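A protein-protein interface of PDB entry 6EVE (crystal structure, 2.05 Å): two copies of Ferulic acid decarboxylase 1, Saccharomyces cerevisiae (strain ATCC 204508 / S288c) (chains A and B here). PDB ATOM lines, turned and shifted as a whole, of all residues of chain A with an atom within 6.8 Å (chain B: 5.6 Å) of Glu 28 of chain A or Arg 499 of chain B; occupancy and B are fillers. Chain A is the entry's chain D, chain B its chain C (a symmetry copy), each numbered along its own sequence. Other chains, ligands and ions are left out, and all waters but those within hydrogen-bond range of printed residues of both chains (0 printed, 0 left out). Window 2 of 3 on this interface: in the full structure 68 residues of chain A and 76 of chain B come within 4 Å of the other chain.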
ATOM      1  N   GLU A  25       3.739   5.243 -27.792  1.00  0.00           N
ATOM      2  CA  GLU A  25       2.767   5.213 -26.691  1.00  0.00           C
ATOM      3  C   GLU A  25       2.287   3.806 -26.575  1.00  0.00           C
ATOM      4  O   GLU A  25       1.604   3.360 -27.460  1.00  0.00           O
ATOM      5  CB  GLU A  25       1.547   6.092 -26.965  1.00  0.00           C
ATOM      6  CG  GLU A  25       1.860   7.548 -27.258  1.00  0.00           C
ATOM      7  CD  GLU A  25       0.695   8.455 -26.935  1.00  0.00           C
ATOM      8  OE1 GLU A  25       0.173   8.385 -25.791  1.00  0.00           O
ATOM      9  OE2 GLU A  25       0.310   9.243 -27.825  1.00  0.00           O
ATOM     10  N   ILE A  26       2.641   3.120 -25.491  1.00  0.00           N
ATOM     11  CA  ILE A  26       2.202   1.758 -25.267  1.00  0.00           C
ATOM     12  C   ILE A  26       0.972   1.743 -24.396  1.00  0.00           C
ATOM     13  O   ILE A  26       1.025   2.130 -23.233  1.00  0.00           O
ATOM     14  CB  ILE A  26       3.272   0.910 -24.623  1.00  0.00           C
ATOM     15  CG1 ILE A  26       4.559   1.050 -25.451  1.00  0.00           C
ATOM     16  CG2 ILE A  26       2.747  -0.518 -24.513  1.00  0.00           C
ATOM     17  CD1 ILE A  26       5.692   0.095 -25.115  1.00  0.00           C
ATOM     18  N   THR A  27      -0.128   1.268 -24.985  1.00  0.00           N
ATOM     19  CA  THR A  27      -1.487   1.367 -24.412  1.00  0.00           C
ATOM     20  C   THR A  27      -1.897   0.068 -23.719  1.00  0.00           C
ATOM     21  O   THR A  27      -2.666   0.111 -22.779  1.00  0.00           O
ATOM     22  CB  THR A  27      -2.540   1.694 -25.493  1.00  0.00           C
ATOM     23  OG1 THR A  27      -2.779   0.528 -26.277  1.00  0.00           O
ATOM     24  CG2 THR A  27      -2.093   2.809 -26.416  1.00  0.00           C
ATOM     25  N   GLU A  28      -1.381  -1.083 -24.150  1.00  0.00           N
ATOM     26  CA  GLU A  28      -1.681  -2.323 -23.425  1.00  0.00           C
ATOM     27  C   GLU A  28      -1.096  -2.331 -21.980  1.00  0.00           C
ATOM     28  O   GLU A  28      -0.267  -1.479 -21.651  1.00  0.00           O
ATOM     29  CB  GLU A  28      -1.261  -3.539 -24.244  1.00  0.00           C
ATOM     30  CG  GLU A  28       0.166  -4.019 -24.075  1.00  0.00           C
ATOM     31  CD  GLU A  28       0.497  -5.174 -25.016  1.00  0.00           C
ATOM     32  OE1 GLU A  28       0.436  -4.950 -26.242  1.00  0.00           O
ATOM     33  OE2 GLU A  28       0.813  -6.295 -24.540  1.00  0.00           O
ATOM     34  N   GLU A  29      -1.542  -3.260 -21.129  1.00  0.00           N
ATOM     35  CA  GLU A  29      -1.140  -3.280 -19.710  1.00  0.00           C
ATOM     36  C   GLU A  29       0.247  -3.876 -19.612  1.00  0.00           C
ATOM     37  O   GLU A  29       0.507  -4.922 -20.192  1.00  0.00           O
ATOM     38  CB  GLU A  29      -2.092  -4.075 -18.802  1.00  0.00           C
ATOM     39  CG  GLU A  29      -1.480  -4.421 -17.443  1.00  0.00           C
ATOM     40  CD  GLU A  29      -2.470  -4.945 -16.410  1.00  0.00           C
ATOM     41  OE1 GLU A  29      -3.479  -4.267 -16.131  1.00  0.00           O
ATOM     42  OE2 GLU A  29      -2.207  -6.026 -15.844  1.00  0.00           O
ATOM     43  N   ILE A  30       1.116  -3.206 -18.853  1.00  0.00           N
ATOM     44  CA  ILE A  30       2.529  -3.588 -18.700  1.00  0.00           C
ATOM     45  C   ILE A  30       2.793  -3.639 -17.196  1.00  0.00           C
ATOM     46  O   ILE A  30       2.465  -2.702 -16.485  1.00  0.00           O
ATOM     47  CB  ILE A  30       3.466  -2.550 -19.392  1.00  0.00           C
ATOM     48  CG1 ILE A  30       3.264  -2.503 -20.918  1.00  0.00           C
ATOM     49  CG2 ILE A  30       4.943  -2.828 -19.082  1.00  0.00           C
ATOM     50  CD1 ILE A  30       3.714  -3.760 -21.669  1.00  0.00           C
ATOM     51  N   GLU A  35       8.996  -5.816 -16.447  1.00  0.00           N
ATOM     52  CA  GLU A  35       8.638  -5.652 -17.847  1.00  0.00           C
ATOM     53  C   GLU A  35       9.018  -4.291 -18.385  1.00  0.00           C
ATOM     54  O   GLU A  35       9.543  -4.199 -19.505  1.00  0.00           O
ATOM     55  CB  GLU A  35       7.150  -5.846 -18.112  1.00  0.00           C
ATOM     56  CG  GLU A  35       6.618  -7.263 -18.020  1.00  0.00           C
ATOM     57  CD  GLU A  35       5.138  -7.372 -18.474  1.00  0.00           C
ATOM     58  OE1 GLU A  35       4.576  -6.388 -19.043  1.00  0.00           O
ATOM     59  OE2 GLU A  35       4.535  -8.453 -18.251  1.00  0.00           O
ATOM     60  N   PHE A  53       4.950   4.362 -21.387  1.00  0.00           N
ATOM     61  CA  PHE A  53       4.066   3.351 -20.773  1.00  0.00           C
ATOM     62  C   PHE A  53       2.805   4.013 -20.169  1.00  0.00           C
ATOM     63  O   PHE A  53       2.865   4.625 -19.111  1.00  0.00           O
ATOM     64  CB  PHE A  53       4.777   2.538 -19.647  1.00  0.00           C
ATOM     65  CG  PHE A  53       6.060   1.886 -20.066  1.00  0.00           C
ATOM     66  CD1 PHE A  53       6.054   0.628 -20.608  1.00  0.00           C
ATOM     67  CD2 PHE A  53       7.255   2.549 -19.950  1.00  0.00           C
ATOM     68  CE1 PHE A  53       7.227   0.020 -21.016  1.00  0.00           C
ATOM     69  CE2 PHE A  53       8.436   1.953 -20.352  1.00  0.00           C
ATOM     70  CZ  PHE A  53       8.413   0.690 -20.887  1.00  0.00           C
ATOM     71  N   LYS A  54       1.674   3.861 -20.852  1.00  0.00           N
ATOM     72  CA  LYS A  54       0.462   4.587 -20.539  1.00  0.00           C
ATOM     73  C   LYS A  54      -0.471   3.837 -19.605  1.00  0.00           C
ATOM     74  O   LYS A  54      -1.361   4.452 -19.023  1.00  0.00           O
ATOM     75  CB  LYS A  54      -0.305   4.932 -21.827  1.00  0.00           C
ATOM     76  CG  LYS A  54       0.332   6.063 -22.595  1.00  0.00           C
ATOM     77  CD  LYS A  54       0.004   7.415 -21.982  1.00  0.00           C
ATOM     78  CE  LYS A  54      -1.125   8.120 -22.720  1.00  0.00           C
ATOM     79  NZ  LYS A  54      -0.777   9.553 -22.923  1.00  0.00           N
ATOM     80  N   ASN A  55      -0.305   2.531 -19.472  1.00  0.00           N
ATOM     81  CA  ASN A  55      -1.226   1.776 -18.692  1.00  0.00           C
ATOM     82  C   ASN A  55      -0.450   0.750 -17.880  1.00  0.00           C
ATOM     83  O   ASN A  55      -0.411  -0.415 -18.200  1.00  0.00           O
ATOM     84  CB  ASN A  55      -2.277   1.172 -19.646  1.00  0.00           C
ATOM     85  CG  ASN A  55      -3.130   0.078 -19.009  1.00  0.00           C
ATOM     86  OD1 ASN A  55      -3.327   0.034 -17.791  1.00  0.00           O
ATOM     87  ND2 ASN A  55      -3.577  -0.853 -19.831  1.00  0.00           N
ATOM     88  N   LEU A  56       0.147   1.223 -16.791  1.00  0.00           N
ATOM     89  CA  LEU A  56       0.868   0.381 -15.840  1.00  0.00           C
ATOM     90  C   LEU A  56      -0.069  -0.293 -14.891  1.00  0.00           C
ATOM     91  O   LEU A  56      -0.903   0.354 -14.261  1.00  0.00           O
ATOM     92  CB  LEU A  56       1.831   1.213 -14.994  1.00  0.00           C
ATOM     93  CG  LEU A  56       3.020   1.845 -15.687  1.00  0.00           C
ATOM     94  CD1 LEU A  56       3.773   2.692 -14.685  1.00  0.00           C
ATOM     95  CD2 LEU A  56       3.926   0.753 -16.231  1.00  0.00           C
ATOM     96  N   GLU B 495       7.971 -11.189 -28.732  1.00  0.00           N
ATOM     97  CA  GLU B 495       6.622 -11.467 -29.312  1.00  0.00           C
ATOM     98  C   GLU B 495       5.711 -10.278 -29.487  1.00  0.00           C
ATOM     99  O   GLU B 495       5.009 -10.196 -30.483  1.00  0.00           O
ATOM    100  CB  GLU B 495       5.824 -12.361 -28.397  1.00  0.00           C
ATOM    101  CG  GLU B 495       5.863 -13.852 -28.616  1.00  0.00           C
ATOM    102  CD  GLU B 495       4.956 -14.530 -27.592  1.00  0.00           C
ATOM    103  OE1 GLU B 495       3.719 -14.264 -27.616  1.00  0.00           O
ATOM    104  OE2 GLU B 495       5.486 -15.274 -26.730  1.00  0.00           O
ATOM    105  N   ASN B 496       5.647  -9.404 -28.480  1.00  0.00           N
ATOM    106  CA  ASN B 496       4.645  -8.284 -28.436  1.00  0.00           C
ATOM    107  C   ASN B 496       5.147  -6.954 -28.987  1.00  0.00           C
ATOM    108  O   ASN B 496       4.383  -5.948 -29.020  1.00  0.00           O
ATOM    109  CB  ASN B 496       4.123  -8.137 -27.005  1.00  0.00           C
ATOM    110  CG  ASN B 496       3.311  -9.341 -26.571  1.00  0.00           C
ATOM    111  OD1 ASN B 496       2.514  -9.825 -27.336  1.00  0.00           O
ATOM    112  ND2 ASN B 496       3.504  -9.818 -25.360  1.00  0.00           N
ATOM    113  N   TRP B 497       6.389  -6.997 -29.514  1.00  0.00           N
ATOM    114  CA  TRP B 497       7.138  -5.819 -29.979  1.00  0.00           C
ATOM    115  C   TRP B 497       6.397  -5.005 -31.049  1.00  0.00           C
ATOM    116  O   TRP B 497       6.321  -3.758 -30.984  1.00  0.00           O
ATOM    117  CB  TRP B 497       8.577  -6.217 -30.438  1.00  0.00           C
ATOM    118  CG  TRP B 497       9.569  -5.051 -30.328  1.00  0.00           C
ATOM    119  CD1 TRP B 497      10.217  -4.421 -31.346  1.00  0.00           C
ATOM    120  CD2 TRP B 497       9.961  -4.358 -29.118  1.00  0.00           C
ATOM    121  NE1 TRP B 497      10.993  -3.381 -30.856  1.00  0.00           N
ATOM    122  CE2 TRP B 497      10.856  -3.325 -29.497  1.00  0.00           C
ATOM    123  CE3 TRP B 497       9.651  -4.521 -27.759  1.00  0.00           C
ATOM    124  CZ2 TRP B 497      11.428  -2.453 -28.570  1.00  0.00           C
ATOM    125  CZ3 TRP B 497      10.215  -3.644 -26.823  1.00  0.00           C
ATOM    126  CH2 TRP B 497      11.105  -2.635 -27.239  1.00  0.00           C
ATOM    127  N   LYS B 498       5.825  -5.729 -32.002  1.00  0.00           N
ATOM    128  CA  LYS B 498       4.995  -5.163 -33.056  1.00  0.00           C
ATOM    129  C   LYS B 498       3.725  -4.553 -32.512  1.00  0.00           C
ATOM    130  O   LYS B 498       3.401  -3.429 -32.852  1.00  0.00           O
ATOM    131  N   ARG B 499       3.002  -5.306 -31.682  1.00  0.00           N
ATOM    132  CA  ARG B 499       1.720  -4.859 -31.117  1.00  0.00           C
ATOM    133  C   ARG B 499       1.835  -3.601 -30.247  1.00  0.00           C
ATOM    134  O   ARG B 499       0.899  -2.766 -30.210  1.00  0.00           O
ATOM    135  CB  ARG B 499       1.062  -5.972 -30.311  1.00  0.00           C
ATOM    136  CG  ARG B 499      -0.299  -5.561 -29.700  1.00  0.00           C
ATOM    137  CD  ARG B 499      -1.025  -6.736 -29.076  1.00  0.00           C
ATOM    138  NE  ARG B 499      -0.463  -7.088 -27.766  1.00  0.00           N
ATOM    139  CZ  ARG B 499      -0.506  -8.293 -27.191  1.00  0.00           C
ATOM    140  NH1 ARG B 499      -1.064  -9.329 -27.795  1.00  0.00           N
ATOM    141  NH2 ARG B 499       0.046  -8.475 -25.996  1.00  0.00           N
ATOM    142  N   TYR B 500       2.965  -3.489 -29.535  1.00  0.00           N
ATOM    143  CA  TYR B 500       3.297  -2.280 -28.752  1.00  0.00           C
ATOM    144  C   TYR B 500       3.362  -1.019 -29.629  1.00  0.00           C
ATOM    145  O   TYR B 500       2.994   0.082 -29.206  1.00  0.00           O
ATOM    146  CB  TYR B 500       4.652  -2.450 -28.055  1.00  0.00           C
ATOM    147  CG  TYR B 500       4.815  -3.554 -27.004  1.00  0.00           C
ATOM    148  CD1 TYR B 500       3.736  -4.079 -26.292  1.00  0.00           C
ATOM    149  CD2 TYR B 500       6.085  -4.020 -26.681  1.00  0.00           C
ATOM    150  CE1 TYR B 500       3.906  -5.056 -25.319  1.00  0.00           C
ATOM    151  CE2 TYR B 500       6.261  -4.994 -25.711  1.00  0.00           C
ATOM    152  CZ  TYR B 500       5.164  -5.490 -25.042  1.00  0.00           C
ATOM    153  OH  TYR B 500       5.339  -6.429 -24.109  1.00  0.00           O
ATOM    154  N   GLY B 501       3.846  -1.172 -30.855  1.00  0.00           N
ATOM    155  CA  GLY B 501       3.915  -0.037 -31.777  1.00  0.00           C
ATOM    156  C   GLY B 501       5.221   0.125 -32.518  1.00  0.00           C
ATOM    157  O   GLY B 501       5.300   1.006 -33.356  1.00  0.00           O
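Of the 7 printed residues of chain B, 2 touch a printed residue of chain A.
Hydrophobic or aromatic side chains of chain B that line the printed part of chain A: Tyr 500.
Of the 11 printed residues of chain A, 3 touch a printed residue of chain B.
Hydrophobic or aromatic side chains of chain A within 4 Å of the printed part of chain B: Ile 30.
Among the printed residues, 4 pairs touch across the chains.
Among the printed residues, Asp or Glu carboxylates within 4 Å of a Lys or Arg side-chain nitrogen of the other chain: Glu 28 of chain A with Arg 499 of chain B (2.7 Å).
NZ of Lys 54 of chain A is in salt-bridge range of OE1 of Glu 25 of chain A (3.2 Å).
N of Ile 30 of chain A is in hydrogen-bond range of O of Asn 55 of chain A, 3.2 Å away.
The side-chain amide oxygen (OD1) of Asn 496 of chain B lies within hydrogen-bond range of the guanidinium group (NH2) of Arg 499 of chain B (3.1 Å).
Arg 499 of chain B touches just one residue of chain A: Glu 28 (2.7 Å).
Printed residues of chain A within 4 Å of Tyr 500 of chain B: Glu 25, Glu 28 and Ile 30.
Of the printed residues of chain B, Ile 30 of chain A touches Tyr 500.
Of the printed residues of chain B, Glu 25 of chain A touches Tyr 500.
Gly 501 of chain B touches none of the printed residues of chain A.
The nearest residue of chain B that does not touch Glu 28 of chain A is Asn 496 of chain B (4.4 Å).
The nearest residue of chain A that does not touch Arg 499 of chain B is Thr 27 of chain A (6.3 Å).
The side-chain carboxylate of Glu 28 of chain A lies within salt-bridge range of the guanidinium group of Arg 499 of chain B (2.7 Å).
No position is printed for both chains.
Of the 4 pairs that touch across the chains among the printed residues, none has its exchanged pair printed and touching as well.
Among the printed residues, merely in contact across the chains: Glu 25 of chain A with Tyr 500 of chain B, Glu 28 of chain A with Tyr 500 of chain B and Ile 30 of chain A with Tyr 500 of chain B.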
